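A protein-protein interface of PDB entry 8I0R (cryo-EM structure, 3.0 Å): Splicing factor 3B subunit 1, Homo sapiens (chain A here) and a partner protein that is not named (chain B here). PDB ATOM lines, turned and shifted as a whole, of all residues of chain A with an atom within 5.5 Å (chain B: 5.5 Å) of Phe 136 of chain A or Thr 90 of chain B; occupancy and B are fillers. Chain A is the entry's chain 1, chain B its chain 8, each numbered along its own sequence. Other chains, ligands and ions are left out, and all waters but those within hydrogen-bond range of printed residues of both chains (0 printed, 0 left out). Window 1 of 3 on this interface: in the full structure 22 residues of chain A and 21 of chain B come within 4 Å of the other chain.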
ATOM      1  N   ASP A 134      -3.454 -19.581  31.672  1.00  0.00           N
ATOM      2  CA  ASP A 134      -3.832 -18.201  31.410  1.00  0.00           C
ATOM      3  C   ASP A 134      -4.889 -18.167  30.313  1.00  0.00           C
ATOM      4  O   ASP A 134      -4.769 -18.894  29.324  1.00  0.00           O
ATOM      5  CB  ASP A 134      -2.608 -17.383  31.014  1.00  0.00           C
ATOM      6  CG  ASP A 134      -2.818 -16.572  29.760  1.00  0.00           C
ATOM      7  OD1 ASP A 134      -3.716 -15.706  29.729  1.00  0.00           O
ATOM      8  OD2 ASP A 134      -2.066 -16.802  28.796  1.00  0.00           O
ATOM      9  N   PRO A 135      -5.919 -17.354  30.447  1.00  0.00           N
ATOM     10  CA  PRO A 135      -7.039 -17.429  29.504  1.00  0.00           C
ATOM     11  C   PRO A 135      -6.792 -16.653  28.226  1.00  0.00           C
ATOM     12  O   PRO A 135      -7.491 -16.852  27.231  1.00  0.00           O
ATOM     13  CB  PRO A 135      -8.206 -16.824  30.294  1.00  0.00           C
ATOM     14  CG  PRO A 135      -7.692 -16.607  31.690  1.00  0.00           C
ATOM     15  CD  PRO A 135      -6.221 -16.469  31.575  1.00  0.00           C
ATOM     16  N   PHE A 136      -5.811 -15.770  28.229  1.00  0.00           N
ATOM     17  CA  PHE A 136      -5.589 -14.929  27.066  1.00  0.00           C
ATOM     18  C   PHE A 136      -4.575 -15.518  26.102  1.00  0.00           C
ATOM     19  O   PHE A 136      -4.069 -14.804  25.232  1.00  0.00           O
ATOM     20  CB  PHE A 136      -5.162 -13.533  27.513  1.00  0.00           C
ATOM     21  CG  PHE A 136      -6.214 -12.815  28.307  1.00  0.00           C
ATOM     22  CD1 PHE A 136      -6.990 -11.842  27.726  1.00  0.00           C
ATOM     23  CD2 PHE A 136      -6.429 -13.122  29.643  1.00  0.00           C
ATOM     24  CE1 PHE A 136      -7.950 -11.182  28.460  1.00  0.00           C
ATOM     25  CE2 PHE A 136      -7.392 -12.471  30.378  1.00  0.00           C
ATOM     26  CZ  PHE A 136      -8.150 -11.502  29.790  1.00  0.00           C
ATOM     27  N   ALA A 137      -4.290 -16.810  26.224  1.00  0.00           N
ATOM     28  CA  ALA A 137      -3.298 -17.442  25.369  1.00  0.00           C
ATOM     29  C   ALA A 137      -3.951 -17.965  24.098  1.00  0.00           C
ATOM     30  O   ALA A 137      -5.073 -18.480  24.124  1.00  0.00           O
ATOM     31  CB  ALA A 137      -2.604 -18.577  26.116  1.00  0.00           C
ATOM     32  N   ASP A 138      -3.221 -17.853  22.987  1.00  0.00           N
ATOM     33  CA  ASP A 138      -3.768 -17.993  21.638  1.00  0.00           C
ATOM     34  C   ASP A 138      -4.993 -17.093  21.464  1.00  0.00           C
ATOM     35  O   ASP A 138      -6.105 -17.551  21.196  1.00  0.00           O
ATOM     36  CB  ASP A 138      -4.104 -19.455  21.331  1.00  0.00           C
ATOM     37  CG  ASP A 138      -4.353 -19.712  19.851  1.00  0.00           C
ATOM     38  OD1 ASP A 138      -3.763 -20.672  19.323  1.00  0.00           O
ATOM     39  OD2 ASP A 138      -5.131 -18.976  19.211  1.00  0.00           O
ATOM     40  N   GLY A 139      -4.766 -15.792  21.666  1.00  0.00           N
ATOM     41  CA  GLY A 139      -5.734 -14.749  21.372  1.00  0.00           C
ATOM     42  C   GLY A 139      -7.152 -15.042  21.808  1.00  0.00           C
ATOM     43  O   GLY A 139      -8.105 -14.518  21.228  1.00  0.00           O
ATOM     44  N   GLY A 140      -7.304 -15.880  22.826  1.00  0.00           N
ATOM     45  CA  GLY A 140      -8.608 -16.391  23.186  1.00  0.00           C
ATOM     46  C   GLY A 140      -8.965 -17.653  22.431  1.00  0.00           C
ATOM     47  O   GLY A 140      -9.978 -17.699  21.729  1.00  0.00           O
ATOM     48  N   ARG A 568       1.493 -13.349  33.114  1.00  0.00           N
ATOM     49  CA  ARG A 568       0.060 -13.602  33.236  1.00  0.00           C
ATOM     50  C   ARG A 568      -0.295 -14.909  33.937  1.00  0.00           C
ATOM     51  O   ARG A 568      -1.367 -14.989  34.540  1.00  0.00           O
ATOM     52  CB  ARG A 568      -0.605 -13.595  31.861  1.00  0.00           C
ATOM     53  CG  ARG A 568      -0.810 -12.238  31.233  1.00  0.00           C
ATOM     54  CD  ARG A 568      -1.751 -12.351  30.047  1.00  0.00           C
ATOM     55  NE  ARG A 568      -1.797 -11.136  29.238  1.00  0.00           N
ATOM     56  CZ  ARG A 568      -2.371 -10.001  29.614  1.00  0.00           C
ATOM     57  NH1 ARG A 568      -2.952  -9.905  30.796  1.00  0.00           N
ATOM     58  NH2 ARG A 568      -2.359  -8.956  28.804  1.00  0.00           N
ATOM     59  N   ALA A 607      -8.309  -7.556  34.120  1.00  0.00           N
ATOM     60  CA  ALA A 607      -9.052  -8.809  34.126  1.00  0.00           C
ATOM     61  C   ALA A 607      -8.263  -9.931  34.774  1.00  0.00           C
ATOM     62  O   ALA A 607      -8.820 -10.733  35.532  1.00  0.00           O
ATOM     63  CB  ALA A 607      -9.436  -9.189  32.704  1.00  0.00           C
ATOM     64  N   THR A 608      -6.960  -9.996  34.510  1.00  0.00           N
ATOM     65  CA  THR A 608      -6.132 -10.995  35.172  1.00  0.00           C
ATOM     66  C   THR A 608      -6.168 -10.823  36.680  1.00  0.00           C
ATOM     67  O   THR A 608      -6.371 -11.792  37.415  1.00  0.00           O
ATOM     68  CB  THR A 608      -4.699 -10.927  34.663  1.00  0.00           C
ATOM     69  OG1 THR A 608      -4.150  -9.640  34.955  1.00  0.00           O
ATOM     70  CG2 THR A 608      -4.666 -11.148  33.180  1.00  0.00           C
ATOM     71  N   LEU B  24      -5.128  -5.666  24.241  1.00  0.00           N
ATOM     72  CA  LEU B  24      -6.109  -6.718  23.983  1.00  0.00           C
ATOM     73  C   LEU B  24      -7.146  -6.258  22.969  1.00  0.00           C
ATOM     74  O   LEU B  24      -7.647  -7.056  22.167  1.00  0.00           O
ATOM     75  CB  LEU B  24      -6.799  -7.133  25.276  1.00  0.00           C
ATOM     76  CG  LEU B  24      -5.891  -7.529  26.429  1.00  0.00           C
ATOM     77  CD1 LEU B  24      -6.363  -6.866  27.708  1.00  0.00           C
ATOM     78  CD2 LEU B  24      -5.862  -9.015  26.553  1.00  0.00           C
ATOM     79  N   LEU B  28      -7.350  -9.431  20.508  1.00  0.00           N
ATOM     80  CA  LEU B  28      -8.209 -10.539  20.894  1.00  0.00           C
ATOM     81  C   LEU B  28      -9.163 -10.893  19.750  1.00  0.00           C
ATOM     82  O   LEU B  28      -9.307 -10.148  18.775  1.00  0.00           O
ATOM     83  CB  LEU B  28      -8.978 -10.191  22.169  1.00  0.00           C
ATOM     84  CG  LEU B  28      -9.665 -11.308  22.959  1.00  0.00           C
ATOM     85  CD1 LEU B  28      -8.640 -12.279  23.505  1.00  0.00           C
ATOM     86  CD2 LEU B  28     -10.529 -10.750  24.084  1.00  0.00           C
ATOM     87  N   MET B  85     -16.790  -5.736  28.323  1.00  0.00           N
ATOM     88  CA  MET B  85     -17.476  -6.756  29.099  1.00  0.00           C
ATOM     89  C   MET B  85     -16.975  -8.145  28.751  1.00  0.00           C
ATOM     90  O   MET B  85     -16.782  -8.978  29.645  1.00  0.00           O
ATOM     91  CB  MET B  85     -18.979  -6.654  28.885  1.00  0.00           C
ATOM     92  CG  MET B  85     -19.788  -7.551  29.791  1.00  0.00           C
ATOM     93  SD  MET B  85     -21.473  -6.958  29.958  1.00  0.00           S
ATOM     94  CE  MET B  85     -21.524  -5.729  28.655  1.00  0.00           C
ATOM     95  N   GLN B  86     -16.728  -8.406  27.471  1.00  0.00           N
ATOM     96  CA  GLN B  86     -16.197  -9.707  27.085  1.00  0.00           C
ATOM     97  C   GLN B  86     -14.815  -9.918  27.675  1.00  0.00           C
ATOM     98  O   GLN B  86     -14.495 -11.003  28.174  1.00  0.00           O
ATOM     99  CB  GLN B  86     -16.161  -9.828  25.568  1.00  0.00           C
ATOM    100  CG  GLN B  86     -16.230 -11.242  25.081  1.00  0.00           C
ATOM    101  CD  GLN B  86     -15.575 -11.386  23.742  1.00  0.00           C
ATOM    102  OE1 GLN B  86     -15.388 -10.407  23.025  1.00  0.00           O
ATOM    103  NE2 GLN B  86     -15.175 -12.597  23.411  1.00  0.00           N
ATOM    104  N   ILE B  87     -13.984  -8.878  27.644  1.00  0.00           N
ATOM    105  CA  ILE B  87     -12.684  -8.963  28.296  1.00  0.00           C
ATOM    106  C   ILE B  87     -12.853  -9.350  29.756  1.00  0.00           C
ATOM    107  O   ILE B  87     -12.363 -10.391  30.201  1.00  0.00           O
ATOM    108  CB  ILE B  87     -11.917  -7.643  28.159  1.00  0.00           C
ATOM    109  CG1 ILE B  87     -11.588  -7.377  26.695  1.00  0.00           C
ATOM    110  CG2 ILE B  87     -10.670  -7.703  28.987  1.00  0.00           C
ATOM    111  CD1 ILE B  87     -10.596  -6.257  26.487  1.00  0.00           C
ATOM    112  N   ASN B  88     -13.575  -8.524  30.517  1.00  0.00           N
ATOM    113  CA  ASN B  88     -13.727  -8.759  31.948  1.00  0.00           C
ATOM    114  C   ASN B  88     -14.277 -10.135  32.268  1.00  0.00           C
ATOM    115  O   ASN B  88     -13.983 -10.685  33.331  1.00  0.00           O
ATOM    116  CB  ASN B  88     -14.625  -7.698  32.556  1.00  0.00           C
ATOM    117  CG  ASN B  88     -13.860  -6.493  32.987  1.00  0.00           C
ATOM    118  OD1 ASN B  88     -12.771  -6.235  32.489  1.00  0.00           O
ATOM    119  ND2 ASN B  88     -14.414  -5.738  33.916  1.00  0.00           N
ATOM    120  N   LEU B  89     -15.082 -10.711  31.381  1.00  0.00           N
ATOM    121  CA  LEU B  89     -15.567 -12.053  31.674  1.00  0.00           C
ATOM    122  C   LEU B  89     -14.598 -13.119  31.203  1.00  0.00           C
ATOM    123  O   LEU B  89     -14.754 -14.291  31.562  1.00  0.00           O
ATOM    124  CB  LEU B  89     -16.931 -12.291  31.039  1.00  0.00           C
ATOM    125  CG  LEU B  89     -18.063 -11.336  31.385  1.00  0.00           C
ATOM    126  CD1 LEU B  89     -19.360 -12.087  31.292  1.00  0.00           C
ATOM    127  CD2 LEU B  89     -17.894 -10.744  32.771  1.00  0.00           C
ATOM    128  N   THR B  90     -13.619 -12.745  30.376  1.00  0.00           N
ATOM    129  CA  THR B  90     -12.675 -13.734  29.872  1.00  0.00           C
ATOM    130  C   THR B  90     -11.913 -14.428  30.984  1.00  0.00           C
ATOM    131  O   THR B  90     -11.556 -15.599  30.851  1.00  0.00           O
ATOM    132  CB  THR B  90     -11.690 -13.079  28.923  1.00  0.00           C
ATOM    133  OG1 THR B  90     -12.356 -12.026  28.227  1.00  0.00           O
ATOM    134  CG2 THR B  90     -11.193 -14.077  27.935  1.00  0.00           C
ATOM    135  N   GLY B  91     -11.631 -13.726  32.076  1.00  0.00           N
ATOM    136  CA  GLY B  91     -10.968 -14.378  33.188  1.00  0.00           C
ATOM    137  C   GLY B  91     -11.845 -15.437  33.820  1.00  0.00           C
ATOM    138  O   GLY B  91     -11.479 -16.612  33.875  1.00  0.00           O
ATOM    139  N   PHE B  92     -13.028 -15.036  34.278  1.00  0.00           N
ATOM    140  CA  PHE B  92     -13.906 -15.930  35.020  1.00  0.00           C
ATOM    141  C   PHE B  92     -14.356 -17.112  34.180  1.00  0.00           C
ATOM    142  O   PHE B  92     -14.270 -18.260  34.622  1.00  0.00           O
ATOM    143  CB  PHE B  92     -15.117 -15.158  35.524  1.00  0.00           C
ATOM    144  CG  PHE B  92     -14.780 -14.065  36.480  1.00  0.00           C
ATOM    145  CD1 PHE B  92     -14.971 -14.239  37.829  1.00  0.00           C
ATOM    146  CD2 PHE B  92     -14.295 -12.862  36.037  1.00  0.00           C
ATOM    147  CE1 PHE B  92     -14.674 -13.247  38.715  1.00  0.00           C
ATOM    148  CE2 PHE B  92     -14.009 -11.868  36.922  1.00  0.00           C
ATOM    149  CZ  PHE B  92     -14.197 -12.065  38.263  1.00  0.00           C
ATOM    150  N   LEU B  93     -14.842 -16.858  32.979  1.00  0.00           N
ATOM    151  CA  LEU B  93     -15.174 -17.940  32.071  1.00  0.00           C
ATOM    152  C   LEU B  93     -13.916 -18.306  31.292  1.00  0.00           C
ATOM    153  O   LEU B  93     -12.834 -17.770  31.535  1.00  0.00           O
ATOM    154  CB  LEU B  93     -16.346 -17.534  31.189  1.00  0.00           C
ATOM    155  CG  LEU B  93     -17.479 -16.932  32.018  1.00  0.00           C
ATOM    156  CD1 LEU B  93     -18.549 -16.339  31.126  1.00  0.00           C
ATOM    157  CD2 LEU B  93     -18.056 -17.983  32.950  1.00  0.00           C
ATOM    158  N   ASN B  94     -14.031 -19.240  30.357  1.00  0.00           N
ATOM    159  CA  ASN B  94     -12.820 -19.801  29.783  1.00  0.00           C
ATOM    160  C   ASN B  94     -12.426 -19.164  28.464  1.00  0.00           C
ATOM    161  O   ASN B  94     -11.775 -19.825  27.653  1.00  0.00           O
ATOM    162  CB  ASN B  94     -12.989 -21.304  29.614  1.00  0.00           C
ATOM    163  CG  ASN B  94     -13.420 -21.978  30.898  1.00  0.00           C
ATOM    164  OD1 ASN B  94     -14.053 -21.359  31.750  1.00  0.00           O
ATOM    165  ND2 ASN B  94     -13.077 -23.248  31.044  1.00  0.00           N
ATOM    166  N   GLY B  95     -12.802 -17.927  28.224  1.00  0.00           N
ATOM    167  CA  GLY B  95     -12.356 -17.218  27.033  1.00  0.00           C
ATOM    168  C   GLY B  95     -13.217 -17.378  25.801  1.00  0.00           C
ATOM    169  O   GLY B  95     -13.763 -16.400  25.290  1.00  0.00           O
ATOM    170  N   ALA B  98     -16.681 -16.943  26.966  1.00  0.00           N
ATOM    171  CA  ALA B  98     -17.054 -15.540  27.069  1.00  0.00           C
ATOM    172  C   ALA B  98     -17.509 -15.001  25.721  1.00  0.00           C
ATOM    173  O   ALA B  98     -18.509 -14.281  25.631  1.00  0.00           O
ATOM    174  CB  ALA B  98     -15.882 -14.728  27.620  1.00  0.00           C
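Pro 135 of chain A touches Thr 90 of chain B.
Phe 136 of chain A touches Leu 24 of chain B.
Thr 90 of chain B touches Phe 136 of chain A (CB to CZ, 3.97 Å).
CD1 of Leu 28 of chain B touches O of Gly 139 of chain A, at 3.2 Å.
Gly 140 of chain A touches Leu 28 of chain B.
Of the 14 printed residues of chain B, 3 touch a printed residue of chain A.
Of the 10 printed residues of chain A, 4 touch a printed residue of chain B.
The side-chain carboxylate of Asp 134 of chain A is in hydrogen-bond range of the backbone NH of Phe 136 of chain A.
The backbone carbonyl oxygen (O) of Ile 87 of chain B lies within hydrogen-bond range of the side-chain hydroxyl (OG1) of Thr 90 of chain B.
Of chain B, only Leu 24 and Thr 90 come within 4 Å of Phe 136 of chain A.
Of chain A, only Pro 135 and Phe 136 come within 4 Å of Thr 90 of chain B.
Of the printed residues of chain A, Leu 28 of chain B touches Gly 139 (3.2 Å) and Gly 140 (3.9 Å).
Of the printed residues of chain B, Pro 135 of chain A touches Thr 90.
Of the printed residues of chain B, Gly 139 of chain A touches Leu 28.
Printed residues of chain B within 4 Å of Gly 140 of chain A: Leu 28.
Printed residues of chain A within 4 Å of Leu 24 of chain B: Phe 136.
Ala 137 of chain A touches none of the printed residues of chain B.
Leu 89 of chain B touches none of the printed residues of chain A.
The nearest residue of chain B that does not touch Phe 136 of chain A is Ile 87 of chain B (4.4 Å).
The nearest printed residue of chain A that does not touch Thr 90 of chain B is Ala 607 of chain A (5.9 Å).
The nearest printed residue of chain A that does not touch Leu 24 of chain B is Arg 568 of chain A (4.2 Å).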
